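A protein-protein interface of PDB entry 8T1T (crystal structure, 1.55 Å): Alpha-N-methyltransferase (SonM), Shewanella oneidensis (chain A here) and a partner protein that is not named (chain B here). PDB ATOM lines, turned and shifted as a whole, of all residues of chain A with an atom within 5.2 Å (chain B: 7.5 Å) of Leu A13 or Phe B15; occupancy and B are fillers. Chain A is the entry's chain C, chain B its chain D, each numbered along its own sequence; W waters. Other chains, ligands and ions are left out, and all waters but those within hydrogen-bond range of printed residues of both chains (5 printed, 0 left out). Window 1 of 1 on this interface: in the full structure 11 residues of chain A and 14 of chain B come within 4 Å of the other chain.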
ATOM      1  N   LEU A  11      13.081  20.183 -14.114  1.00  0.00           N
ATOM      2  CA  LEU A  11      12.468  18.943 -13.653  1.00  0.00           C
ATOM      3  C   LEU A  11      10.943  19.056 -13.658  1.00  0.00           C
ATOM      4  O   LEU A  11      10.250  18.083 -13.962  1.00  0.00           O
ATOM      5  CB  LEU A  11      12.995  18.619 -12.248  1.00  0.00           C
ATOM      6  CG  LEU A  11      14.364  17.941 -12.187  1.00  0.00           C
ATOM      7  CD1 LEU A  11      14.299  16.536 -12.770  1.00  0.00           C
ATOM      8  CD2 LEU A  11      15.415  18.768 -12.907  1.00  0.00           C
ATOM      9  N   GLN A  12      10.423  20.239 -13.326  1.00  0.00           N
ATOM     10  CA  GLN A  12       8.987  20.449 -13.238  1.00  0.00           C
ATOM     11  C   GLN A  12       8.414  20.742 -14.622  1.00  0.00           C
ATOM     12  O   GLN A  12       9.053  21.368 -15.457  1.00  0.00           O
ATOM     13  CB  GLN A  12       8.657  21.592 -12.273  1.00  0.00           C
ATOM     14  CG  GLN A  12       8.469  21.151 -10.827  1.00  0.00           C
ATOM     15  CD  GLN A  12       7.172  20.405 -10.603  1.00  0.00           C
ATOM     16  OE1 GLN A  12       6.388  20.186 -11.523  1.00  0.00           O
ATOM     17  NE2 GLN A  12       6.932  20.018  -9.361  1.00  0.00           N
ATOM     18  N   LEU A  13       7.171  20.300 -14.835  1.00  0.00           N
ATOM     19  CA  LEU A  13       6.483  20.470 -16.104  1.00  0.00           C
ATOM     20  C   LEU A  13       6.257  21.950 -16.422  1.00  0.00           C
ATOM     21  O   LEU A  13       5.724  22.691 -15.600  1.00  0.00           O
ATOM     22  CB  LEU A  13       5.147  19.725 -16.009  1.00  0.00           C
ATOM     23  CG  LEU A  13       4.166  19.989 -17.150  1.00  0.00           C
ATOM     24  CD1 LEU A  13       4.690  19.413 -18.453  1.00  0.00           C
ATOM     25  CD2 LEU A  13       2.796  19.414 -16.824  1.00  0.00           C
ATOM     26  N   ALA A  14       6.680  22.349 -17.632  1.00  0.00           N
ATOM     27  CA  ALA A  14       6.272  23.580 -18.299  1.00  0.00           C
ATOM     28  C   ALA A  14       6.954  24.827 -17.729  1.00  0.00           C
ATOM     29  O   ALA A  14       7.339  25.712 -18.490  1.00  0.00           O
ATOM     30  CB  ALA A  14       4.770  23.719 -18.273  1.00  0.00           C
ATOM     31  N   GLY A  15       7.078  24.922 -16.400  1.00  0.00           N
ATOM     32  CA  GLY A  15       7.362  26.201 -15.767  1.00  0.00           C
ATOM     33  C   GLY A  15       8.827  26.412 -15.402  1.00  0.00           C
ATOM     34  O   GLY A  15       9.212  27.518 -15.022  1.00  0.00           O
ATOM     35  N   GLN A  16       9.648  25.358 -15.486  1.00  0.00           N
ATOM     36  CA  GLN A  16      11.004  25.426 -14.968  1.00  0.00           C
ATOM     37  C   GLN A  16      12.016  25.620 -16.101  1.00  0.00           C
ATOM     38  O   GLN A  16      13.216  25.701 -15.846  1.00  0.00           O
ATOM     39  CB  GLN A  16      11.308  24.170 -14.152  1.00  0.00           C
ATOM     40  CG  GLN A  16      12.255  24.416 -12.992  1.00  0.00           C
ATOM     41  CD  GLN A  16      12.160  23.332 -11.946  1.00  0.00           C
ATOM     42  OE1 GLN A  16      12.280  22.147 -12.243  1.00  0.00           O
ATOM     43  NE2 GLN A  16      11.918  23.736 -10.709  1.00  0.00           N
ATOM     44  N   PHE A  39       3.283  13.961 -19.945  1.00  0.00           N
ATOM     45  CA  PHE A  39       2.736  15.296 -19.771  1.00  0.00           C
ATOM     46  C   PHE A  39       3.718  16.305 -20.360  1.00  0.00           C
ATOM     47  O   PHE A  39       3.324  17.221 -21.082  1.00  0.00           O
ATOM     48  CB  PHE A  39       2.436  15.567 -18.294  1.00  0.00           C
ATOM     49  CG  PHE A  39       1.284  14.764 -17.738  1.00  0.00           C
ATOM     50  CD1 PHE A  39      -0.015  14.999 -18.162  1.00  0.00           C
ATOM     51  CD2 PHE A  39       1.503  13.763 -16.806  1.00  0.00           C
ATOM     52  CE1 PHE A  39      -1.071  14.260 -17.648  1.00  0.00           C
ATOM     53  CE2 PHE A  39       0.446  13.031 -16.288  1.00  0.00           C
ATOM     54  CZ  PHE A  39      -0.837  13.278 -16.713  1.00  0.00           C
ATOM     55  N   SER A  40       5.001  16.074 -20.087  1.00  0.00           N
ATOM     56  CA  SER A  40       6.062  16.914 -20.611  1.00  0.00           C
ATOM     57  C   SER A  40       6.139  16.770 -22.131  1.00  0.00           C
ATOM     58  O   SER A  40       6.334  17.751 -22.836  1.00  0.00           O
ATOM     59  CB  SER A  40       7.379  16.591 -19.950  1.00  0.00           C
ATOM     60  OG  SER A  40       8.359  17.562 -20.296  1.00  0.00           O
ATOM     61  N   TRP A  43       3.370  18.793 -23.700  1.00  0.00           N
ATOM     62  CA  TRP A  43       3.728  20.193 -23.561  1.00  0.00           C
ATOM     63  C   TRP A  43       4.671  20.605 -24.690  1.00  0.00           C
ATOM     64  O   TRP A  43       4.462  21.624 -25.340  1.00  0.00           O
ATOM     65  CB  TRP A  43       4.353  20.440 -22.183  1.00  0.00           C
ATOM     66  CG  TRP A  43       5.177  21.685 -22.100  1.00  0.00           C
ATOM     67  CD1 TRP A  43       4.730  22.968 -21.996  1.00  0.00           C
ATOM     68  CD2 TRP A  43       6.613  21.764 -22.160  1.00  0.00           C
ATOM     69  NE1 TRP A  43       5.784  23.839 -21.956  1.00  0.00           N
ATOM     70  CE2 TRP A  43       6.951  23.130 -22.063  1.00  0.00           C
ATOM     71  CE3 TRP A  43       7.639  20.819 -22.268  1.00  0.00           C
ATOM     72  CZ2 TRP A  43       8.275  23.571 -22.080  1.00  0.00           C
ATOM     73  CZ3 TRP A  43       8.945  21.254 -22.285  1.00  0.00           C
ATOM     74  CH2 TRP A  43       9.255  22.613 -22.189  1.00  0.00           C
ATOM     75  N   ASN A 210       8.076  16.005 -10.767  1.00  0.00           N
ATOM     76  CA  ASN A 210       8.035  16.343 -12.182  1.00  0.00           C
ATOM     77  C   ASN A 210       6.706  17.006 -12.563  1.00  0.00           C
ATOM     78  O   ASN A 210       6.595  17.570 -13.651  1.00  0.00           O
ATOM     79  CB  ASN A 210       8.280  15.115 -13.060  1.00  0.00           C
ATOM     80  CG  ASN A 210       9.658  14.514 -12.873  1.00  0.00           C
ATOM     81  OD1 ASN A 210      10.670  15.183 -13.080  1.00  0.00           O
ATOM     82  ND2 ASN A 210       9.710  13.252 -12.482  1.00  0.00           N
ATOM     83  N   LEU A 211       5.690  16.898 -11.693  1.00  0.00           N
ATOM     84  CA  LEU A 211       4.381  17.490 -11.946  1.00  0.00           C
ATOM     85  C   LEU A 211       4.044  18.511 -10.860  1.00  0.00           C
ATOM     86  O   LEU A 211       4.446  18.360  -9.708  1.00  0.00           O
ATOM     87  CB  LEU A 211       3.322  16.381 -11.978  1.00  0.00           C
ATOM     88  CG  LEU A 211       3.445  15.376 -13.121  1.00  0.00           C
ATOM     89  CD1 LEU A 211       2.408  14.266 -12.980  1.00  0.00           C
ATOM     90  CD2 LEU A 211       3.310  16.065 -14.472  1.00  0.00           C
ATOM     91  N   PRO A 212       3.264  19.564 -11.200  1.00  0.00           N
ATOM     92  CA  PRO A 212       2.936  20.634 -10.256  1.00  0.00           C
ATOM     93  C   PRO A 212       2.057  20.227  -9.071  1.00  0.00           C
ATOM     94  O   PRO A 212       1.991  20.950  -8.079  1.00  0.00           O
ATOM     95  CB  PRO A 212       2.202  21.666 -11.129  1.00  0.00           C
ATOM     96  CG  PRO A 212       1.671  20.870 -12.304  1.00  0.00           C
ATOM     97  CD  PRO A 212       2.718  19.804 -12.543  1.00  0.00           C
ATOM     98  N   ILE A 213       1.395  19.068  -9.167  1.00  0.00           N
ATOM     99  CA  ILE A 213       0.488  18.613  -8.123  1.00  0.00           C
ATOM    100  C   ILE A 213       1.176  17.567  -7.248  1.00  0.00           C
ATOM    101  O   ILE A 213       0.561  17.012  -6.338  1.00  0.00           O
ATOM    102  CB  ILE A 213      -0.832  18.084  -8.726  1.00  0.00           C
ATOM    103  CG1 ILE A 213      -0.622  17.018  -9.808  1.00  0.00           C
ATOM    104  CG2 ILE A 213      -1.662  19.242  -9.260  1.00  0.00           C
ATOM    105  CD1 ILE A 213       0.097  15.779  -9.346  1.00  0.00           C
ATOM    106  N   SER B   9      -6.743  16.367 -24.118  1.00  0.00           N
ATOM    107  CA  SER B   9      -6.632  15.983 -22.685  1.00  0.00           C
ATOM    108  C   SER B   9      -6.718  17.230 -21.807  1.00  0.00           C
ATOM    109  O   SER B   9      -5.788  18.035 -21.768  1.00  0.00           O
ATOM    110  CB  SER B   9      -5.358  15.215 -22.427  1.00  0.00           C
ATOM    111  OG  SER B   9      -5.225  14.893 -21.049  1.00  0.00           O
ATOM    112  N   GLY B  10      -7.852  17.377 -21.113  1.00  0.00           N
ATOM    113  CA  GLY B  10      -8.046  18.467 -20.172  1.00  0.00           C
ATOM    114  C   GLY B  10      -7.120  18.337 -18.962  1.00  0.00           C
ATOM    115  O   GLY B  10      -6.758  19.336 -18.345  1.00  0.00           O
ATOM    116  N   LEU B  11      -6.747  17.094 -18.641  1.00  0.00           N
ATOM    117  CA  LEU B  11      -5.863  16.810 -17.521  1.00  0.00           C
ATOM    118  C   LEU B  11      -4.484  17.394 -17.818  1.00  0.00           C
ATOM    119  O   LEU B  11      -3.914  18.116 -17.004  1.00  0.00           O
ATOM    120  CB  LEU B  11      -5.792  15.292 -17.324  1.00  0.00           C
ATOM    121  CG  LEU B  11      -5.471  14.818 -15.908  1.00  0.00           C
ATOM    122  CD1 LEU B  11      -4.841  13.433 -15.928  1.00  0.00           C
ATOM    123  CD2 LEU B  11      -4.569  15.805 -15.187  1.00  0.00           C
ATOM    124  N   SER B  12      -3.971  17.083 -19.013  1.00  0.00           N
ATOM    125  CA  SER B  12      -2.675  17.559 -19.462  1.00  0.00           C
ATOM    126  C   SER B  12      -2.674  19.083 -19.563  1.00  0.00           C
ATOM    127  O   SER B  12      -1.726  19.735 -19.131  1.00  0.00           O
ATOM    128  CB  SER B  12      -2.306  16.917 -20.776  1.00  0.00           C
ATOM    129  OG  SER B  12      -1.012  17.320 -21.194  1.00  0.00           O
ATOM    130  N   ASP B  13      -3.744  19.642 -20.143  1.00  0.00           N
ATOM    131  CA  ASP B  13      -3.859  21.081 -20.316  1.00  0.00           C
ATOM    132  C   ASP B  13      -3.794  21.771 -18.955  1.00  0.00           C
ATOM    133  O   ASP B  13      -3.110  22.782 -18.802  1.00  0.00           O
ATOM    134  CB  ASP B  13      -5.144  21.450 -21.063  1.00  0.00           C
ATOM    135  CG  ASP B  13      -5.125  21.110 -22.545  1.00  0.00           C
ATOM    136  OD1 ASP B  13      -4.049  20.728 -23.048  1.00  0.00           O
ATOM    137  OD2 ASP B  13      -6.190  21.231 -23.184  1.00  0.00           O
ATOM    138  N   PHE B  14      -4.505  21.211 -17.969  1.00  0.00           N
ATOM    139  CA  PHE B  14      -4.548  21.784 -16.632  1.00  0.00           C
ATOM    140  C   PHE B  14      -3.155  21.789 -16.001  1.00  0.00           C
ATOM    141  O   PHE B  14      -2.706  22.812 -15.490  1.00  0.00           O
ATOM    142  CB  PHE B  14      -5.538  21.027 -15.742  1.00  0.00           C
ATOM    143  CG  PHE B  14      -5.497  21.447 -14.295  1.00  0.00           C
ATOM    144  CD1 PHE B  14      -5.810  22.746 -13.926  1.00  0.00           C
ATOM    145  CD2 PHE B  14      -5.119  20.555 -13.305  1.00  0.00           C
ATOM    146  CE1 PHE B  14      -5.766  23.136 -12.597  1.00  0.00           C
ATOM    147  CE2 PHE B  14      -5.072  20.949 -11.976  1.00  0.00           C
ATOM    148  CZ  PHE B  14      -5.392  22.240 -11.625  1.00  0.00           C
ATOM    149  N   PHE B  15      -2.473  20.641 -16.031  1.00  0.00           N
ATOM    150  CA  PHE B  15      -1.149  20.529 -15.438  1.00  0.00           C
ATOM    151  C   PHE B  15      -0.188  21.516 -16.100  1.00  0.00           C
ATOM    152  O   PHE B  15       0.634  22.126 -15.420  1.00  0.00           O
ATOM    153  CB  PHE B  15      -0.637  19.090 -15.533  1.00  0.00           C
ATOM    154  CG  PHE B  15      -1.317  18.112 -14.606  1.00  0.00           C
ATOM    155  CD1 PHE B  15      -2.160  18.551 -13.599  1.00  0.00           C
ATOM    156  CD2 PHE B  15      -1.115  16.747 -14.744  1.00  0.00           C
ATOM    157  CE1 PHE B  15      -2.783  17.649 -12.748  1.00  0.00           C
ATOM    158  CE2 PHE B  15      -1.742  15.847 -13.897  1.00  0.00           C
ATOM    159  CZ  PHE B  15      -2.572  16.299 -12.897  1.00  0.00           C
ATOM    160  N   THR B  16      -0.303  21.702 -17.421  1.00  0.00           N
ATOM    161  CA  THR B  16       0.620  22.581 -18.126  1.00  0.00           C
ATOM    162  C   THR B  16       0.405  24.024 -17.672  1.00  0.00           C
ATOM    163  O   THR B  16       1.366  24.755 -17.450  1.00  0.00           O
ATOM    164  CB  THR B  16       0.502  22.439 -19.650  1.00  0.00           C
ATOM    165  OG1 THR B  16       1.057  21.181 -20.038  1.00  0.00           O
ATOM    166  CG2 THR B  16       1.214  23.544 -20.401  1.00  0.00           C
ATOM    167  N   GLN B  17      -0.863  24.429 -17.545  1.00  0.00           N
ATOM    168  CA  GLN B  17      -1.213  25.765 -17.088  1.00  0.00           C
ATOM    169  C   GLN B  17      -0.723  25.976 -15.659  1.00  0.00           C
ATOM    170  O   GLN B  17      -0.079  26.979 -15.352  1.00  0.00           O
ATOM    171  CB  GLN B  17      -2.729  25.977 -17.098  1.00  0.00           C
ATOM    172  CG  GLN B  17      -3.366  25.982 -18.480  1.00  0.00           C
ATOM    173  CD  GLN B  17      -4.873  26.035 -18.389  1.00  0.00           C
ATOM    174  OE1 GLN B  17      -5.443  26.911 -17.742  1.00  0.00           O
ATOM    175  NE2 GLN B  17      -5.534  25.078 -19.022  1.00  0.00           N
ATOM    176  N   LEU B  18      -1.053  25.022 -14.787  1.00  0.00           N
ATOM    177  CA  LEU B  18      -0.719  25.118 -13.373  1.00  0.00           C
ATOM    178  C   LEU B  18       0.790  25.289 -13.203  1.00  0.00           C
ATOM    179  O   LEU B  18       1.245  26.033 -12.336  1.00  0.00           O
ATOM    180  CB  LEU B  18      -1.225  23.854 -12.672  1.00  0.00           C
ATOM    181  CG  LEU B  18      -1.000  23.805 -11.163  1.00  0.00           C
ATOM    182  CD1 LEU B  18      -1.729  24.950 -10.477  1.00  0.00           C
ATOM    183  CD2 LEU B  18      -1.443  22.466 -10.589  1.00  0.00           C
ATOM    184  N   GLY B  19       1.562  24.602 -14.053  1.00  0.00           N
ATOM    185  CA  GLY B  19       3.010  24.589 -13.944  1.00  0.00           C
ATOM    186  C   GLY B  19       3.667  25.903 -14.356  1.00  0.00           C
ATOM    187  O   GLY B  19       4.800  26.152 -13.948  1.00  0.00           O
ATOM    188  N   GLN B  20       2.974  26.734 -15.153  1.00  0.00           N
ATOM    189  CA  GLN B  20       3.583  27.947 -15.687  1.00  0.00           C
ATOM    190  C   GLN B  20       2.966  29.212 -15.093  1.00  0.00           C
ATOM    191  O   GLN B  20       3.545  30.292 -15.206  1.00  0.00           O
ATOM    192  CB  GLN B  20       3.399  28.070 -17.200  1.00  0.00           C
ATOM    193  CG  GLN B  20       3.496  26.769 -17.974  1.00  0.00           C
ATOM    194  CD  GLN B  20       3.123  26.993 -19.419  1.00  0.00           C
ATOM    195  OE1 GLN B  20       3.874  27.589 -20.185  1.00  0.00           O
ATOM    196  NE2 GLN B  20       1.951  26.517 -19.799  1.00  0.00           N
ATOM    197  N   ASP B  21       1.782  29.091 -14.481  1.00  0.00           N
ATOM    198  CA  ASP B  21       0.997  30.257 -14.099  1.00  0.00           C
ATOM    199  C   ASP B  21       0.976  30.378 -12.575  1.00  0.00           C
ATOM    200  O   ASP B  21       0.341  29.581 -11.893  1.00  0.00           O
ATOM    201  CB  ASP B  21      -0.411  30.154 -14.695  1.00  0.00           C
ATOM    202  CG  ASP B  21      -1.356  31.291 -14.351  1.00  0.00           C
ATOM    203  OD1 ASP B  21      -0.962  32.176 -13.569  1.00  0.00           O
ATOM    204  OD2 ASP B  21      -2.491  31.274 -14.877  1.00  0.00           O
ATOM    205  N   LEU B  24      -2.501  30.859 -10.833  1.00  0.00           N
ATOM    206  CA  LEU B  24      -3.247  29.616 -10.750  1.00  0.00           C
ATOM    207  C   LEU B  24      -2.588  28.698  -9.725  1.00  0.00           C
ATOM    208  O   LEU B  24      -3.266  27.986  -8.991  1.00  0.00           O
ATOM    209  CB  LEU B  24      -3.312  28.955 -12.129  1.00  0.00           C
ATOM    210  CG  LEU B  24      -4.027  27.604 -12.164  1.00  0.00           C
ATOM    211  CD1 LEU B  24      -5.440  27.723 -11.619  1.00  0.00           C
ATOM    212  CD2 LEU B  24      -4.050  27.035 -13.578  1.00  0.00           C
ATOM    213  N   MET B  25      -1.255  28.731  -9.664  1.00  0.00           N
ATOM    214  CA  MET B  25      -0.546  27.889  -8.716  1.00  0.00           C
ATOM    215  C   MET B  25      -0.960  28.263  -7.292  1.00  0.00           C
ATOM    216  O   MET B  25      -1.198  27.391  -6.463  1.00  0.00           O
ATOM    217  CB  MET B  25       0.972  28.039  -8.862  1.00  0.00           C
ATOM    218  CG  MET B  25       1.749  27.221  -7.847  1.00  0.00           C
ATOM    219  SD  MET B  25       1.551  25.448  -8.131  1.00  0.00           S
ATOM    220  CE  MET B  25       2.714  25.193  -9.472  1.00  0.00           C
ATOM    221  N   TYR B  28      -4.477  27.225  -6.578  1.00  0.00           N
ATOM    222  CA  TYR B  28      -4.488  25.788  -6.361  1.00  0.00           C
ATOM    223  C   TYR B  28      -4.059  25.458  -4.932  1.00  0.00           C
ATOM    224  O   TYR B  28      -4.660  24.609  -4.279  1.00  0.00           O
ATOM    225  CB  TYR B  28      -3.558  25.081  -7.350  1.00  0.00           C
ATOM    226  CG  TYR B  28      -3.425  23.602  -7.103  1.00  0.00           C
ATOM    227  CD1 TYR B  28      -4.369  22.710  -7.585  1.00  0.00           C
ATOM    228  CD2 TYR B  28      -2.400  23.097  -6.320  1.00  0.00           C
ATOM    229  CE1 TYR B  28      -4.269  21.352  -7.343  1.00  0.00           C
ATOM    230  CE2 TYR B  28      -2.286  21.742  -6.065  1.00  0.00           C
ATOM    231  CZ  TYR B  28      -3.229  20.866  -6.571  1.00  0.00           C
ATOM    232  OH  TYR B  28      -3.121  19.522  -6.320  1.00  0.00           O
ATOM    233  N   MET B  36      -9.333  22.066  -8.925  1.00  0.00           N
ATOM    234  CA  MET B  36      -9.298  20.902  -9.796  1.00  0.00           C
ATOM    235  C   MET B  36     -10.698  20.616 -10.343  1.00  0.00           C
ATOM    236  O   MET B  36     -10.851  20.332 -11.528  1.00  0.00           O
ATOM    237  CB  MET B  36      -8.739  19.686  -9.053  1.00  0.00           C
ATOM    238  CG  MET B  36      -7.222  19.678  -9.035  1.00  0.00           C
ATOM    239  SD  MET B  36      -6.517  18.150  -8.376  1.00  0.00           S
ATOM    240  CE  MET B  36      -6.943  18.286  -6.642  1.00  0.00           C
ATOM    241  N   LEU B  41     -11.588  18.241 -13.690  1.00  0.00           N
ATOM    242  CA  LEU B  41     -10.994  16.953 -13.360  1.00  0.00           C
ATOM    243  C   LEU B  41     -12.052  16.046 -12.734  1.00  0.00           C
ATOM    244  O   LEU B  41     -12.944  16.514 -12.029  1.00  0.00           O
ATOM    245  CB  LEU B  41      -9.806  17.148 -12.414  1.00  0.00           C
ATOM    246  CG  LEU B  41      -8.471  17.477 -13.086  1.00  0.00           C
ATOM    247  CD1 LEU B  41      -8.498  18.864 -13.704  1.00  0.00           C
ATOM    248  CD2 LEU B  41      -7.326  17.359 -12.093  1.00  0.00           C
ATOM    249  N   GLN B  45      -9.479  11.277 -10.848  1.00  0.00           N
ATOM    250  CA  GLN B  45      -8.293  12.078 -11.114  1.00  0.00           C
ATOM    251  C   GLN B  45      -7.908  12.842  -9.848  1.00  0.00           C
ATOM    252  O   GLN B  45      -6.742  12.867  -9.455  1.00  0.00           O
ATOM    253  CB  GLN B  45      -8.538  13.014 -12.301  1.00  0.00           C
ATOM    254  CG  GLN B  45      -8.427  12.320 -13.653  1.00  0.00           C
ATOM    255  CD  GLN B  45      -8.894  13.168 -14.812  1.00  0.00           C
ATOM    256  OE1 GLN B  45      -9.532  14.206 -14.642  1.00  0.00           O
ATOM    257  NE2 GLN B  45      -8.598  12.712 -16.018  1.00  0.00           N
ATOM    258  N   VAL B  49      -4.549  12.536  -7.303  1.00  0.00           N
ATOM    259  CA  VAL B  49      -3.704  13.661  -6.936  1.00  0.00           C
ATOM    260  C   VAL B  49      -3.546  13.700  -5.417  1.00  0.00           C
ATOM    261  O   VAL B  49      -2.440  13.859  -4.905  1.00  0.00           O
ATOM    262  CB  VAL B  49      -4.278  14.991  -7.466  1.00  0.00           C
ATOM    263  CG1 VAL B  49      -3.605  16.192  -6.814  1.00  0.00           C
ATOM    264  CG2 VAL B  49      -4.193  15.087  -8.980  1.00  0.00           C
ATOM    265  N   MET B  54       0.909   8.731  -8.687  1.00  0.00           N
ATOM    266  CA  MET B  54       1.364   9.239  -9.969  1.00  0.00           C
ATOM    267  C   MET B  54       1.126   8.190 -11.054  1.00  0.00           C
ATOM    268  O   MET B  54       0.831   8.528 -12.197  1.00  0.00           O
ATOM    269  CB  MET B  54       2.857   9.585  -9.919  1.00  0.00           C
ATOM    270  CG  MET B  54       3.183  10.805  -9.067  1.00  0.00           C
ATOM    271  SD  MET B  54       2.227  12.282  -9.505  1.00  0.00           S
ATOM    272  CE  MET B  54       0.943  12.229  -8.257  1.00  0.00           C
ATOM    273  N   LEU B  57      -2.449   8.444 -12.302  1.00  0.00           N
ATOM    274  CA  LEU B  57      -2.647   9.673 -13.055  1.00  0.00           C
ATOM    275  C   LEU B  57      -2.276   9.454 -14.519  1.00  0.00           C
ATOM    276  O   LEU B  57      -2.960   9.937 -15.417  1.00  0.00           O
ATOM    277  CB  LEU B  57      -1.791  10.791 -12.451  1.00  0.00           C
ATOM    278  CG  LEU B  57      -2.466  11.634 -11.370  1.00  0.00           C
ATOM    279  CD1 LEU B  57      -1.596  12.826 -11.001  1.00  0.00           C
ATOM    280  CD2 LEU B  57      -3.842  12.099 -11.825  1.00  0.00           C
ATOM    281  N   LYS B  58      -1.173   8.731 -14.742  1.00  0.00           N
ATOM    282  CA  LYS B  58      -0.645   8.526 -16.080  1.00  0.00           C
ATOM    283  C   LYS B  58      -1.536   7.540 -16.831  1.00  0.00           C
ATOM    284  O   LYS B  58      -1.552   7.526 -18.060  1.00  0.00           O
ATOM    285  CB  LYS B  58       0.814   8.067 -15.987  1.00  0.00           C
ATOM    286  CG  LYS B  58       1.746   9.084 -15.340  1.00  0.00           C
ATOM    287  CD  LYS B  58       3.175   8.614 -15.184  1.00  0.00           C
ATOM    288  CE  LYS B  58       4.068   9.672 -14.567  1.00  0.00           C
ATOM    289  NZ  LYS B  58       5.456   9.183 -14.383  1.00  0.00           N
ATOM    290  N   SER B  61      -4.807   9.314 -18.402  1.00  0.00           N
ATOM    291  CA  SER B  61      -4.550  10.223 -19.507  1.00  0.00           C
ATOM    292  C   SER B  61      -4.169   9.423 -20.750  1.00  0.00           C
ATOM    293  O   SER B  61      -4.859   9.481 -21.767  1.00  0.00           O
ATOM    294  CB  SER B  61      -3.488  11.230 -19.147  1.00  0.00           C
ATOM    295  OG  SER B  61      -2.288  10.583 -18.750  1.00  0.00           O
HETATM  296  O   HOH W   1      -1.194  18.610  -4.875  1.00  0.00           O
HETATM  297  O   HOH W   2       6.272  26.635 -20.850  1.00  0.00           O
HETATM  298  O   HOH W   3       1.021  18.394 -19.913  1.00  0.00           O
HETATM  299  O   HOH W   4       3.308  26.055 -22.837  1.00  0.00           O
HETATM  300  O   HOH W   5       0.037  14.456  -5.789  1.00  0.00           O
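Leu A13 touches just these residues of chain B: Phe B15, Thr B16 and Gly B19. Of the printed residues of chain A, Phe B15 touches Leu A13, Phe A39, Pro A212 and Ile A213. Of the printed residues of chain B, Gly A15 touches Gly B19. Printed residues of chain A within 4 Å of Leu B57: Ile A213 (3.8 Å). The nearest residue of chain B that does not touch Leu A13 is Gln B20 (4.9 Å).
Water W1 bridges OH of Tyr B28 and O of Ile A213. Water W3 lies within hydrogen-bond range of the side-chain hydroxyl of Ser B12 (2.6 Å), the side-chain hydroxyl of Thr B16 (2.8 Å) and the backbone carbonyl oxygen of Phe A39 (2.8 Å). Water W2 lies within hydrogen-bond range of the side-chain amide oxygen (OE1) of Gln B20 (2.7 Å), the backbone carbonyl oxygen (O) of Ala A14 (2.7 Å) and the indole nitrogen (NE1) of Trp A43 (3.0 Å). Water W5 bridges the backbone carbonyl oxygen of Ile A213 (2.7 Å) and the backbone carbonyl oxygen of Val B49 (2.7 Å). Water W4 lies within hydrogen-bond range of OE1 of Gln B20 (3.1 Å) and NE1 of Trp A43 (3.4 Å).
N of Leu A13 sits at hydrogen-bond distance from O of Asn A210 (3.0 Å). N of Ser B12 is in hydrogen-bond range of OG of Ser B9 (3.2 Å). O of Ser B12 sits at hydrogen-bond distance from OG1 of Thr B16, at 3.3 Å. The backbone carbonyl oxygen (O) of Thr B16 sits close to the side-chain amide nitrogen (NE2) of Gln B20, 3.0 Å away. O of Leu B57 is in hydrogen-bond range of OG of Ser B61, 3.5 Å away. O of Lys B58 is in hydrogen-bond range of OG of Ser B61.
Printed residues of chain B that touch a printed residue of chain A: Ser B12, Phe B15, Thr B16, Leu B18, Gly B19, Gln B20, Met B25, Tyr B28, Val B49, Met B54, Leu B57 and Ser B61. Hydrophobic or aromatic side chains of chain B that line the printed part of chain A: Phe B15, Leu B18, Met B25, Tyr B28, Val B49, Met B54 and Leu B57. Among the printed residues, 19 pairs touch across the chains. Among the printed residues, no Asp or Glu carboxylate lies within 4 Å of a Lys or Arg side-chain nitrogen of the other chain.
Leu A13 touches Phe B15. CA of Gly B19 touches O of Leu A13, at 3.7 Å. O of Gly B19 touches CA of Gly A15 (3.1 Å). CD1 of Phe A39 touches CA of Ser B12 (3.9 Å). Phe A39 touches Phe B15 (CE1 to CD2, 3.8 Å). Phe A39 touches Ser B61. CG1 of Ile A213 touches CE1 of Phe B15 (3.7 Å). Ile A213 touches Tyr B28 (CG2 to OH, 3.3 Å). Ile A213 touches Val B49 (CB to CG1, 3.9 Å). Ile A213 touches Met B54.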
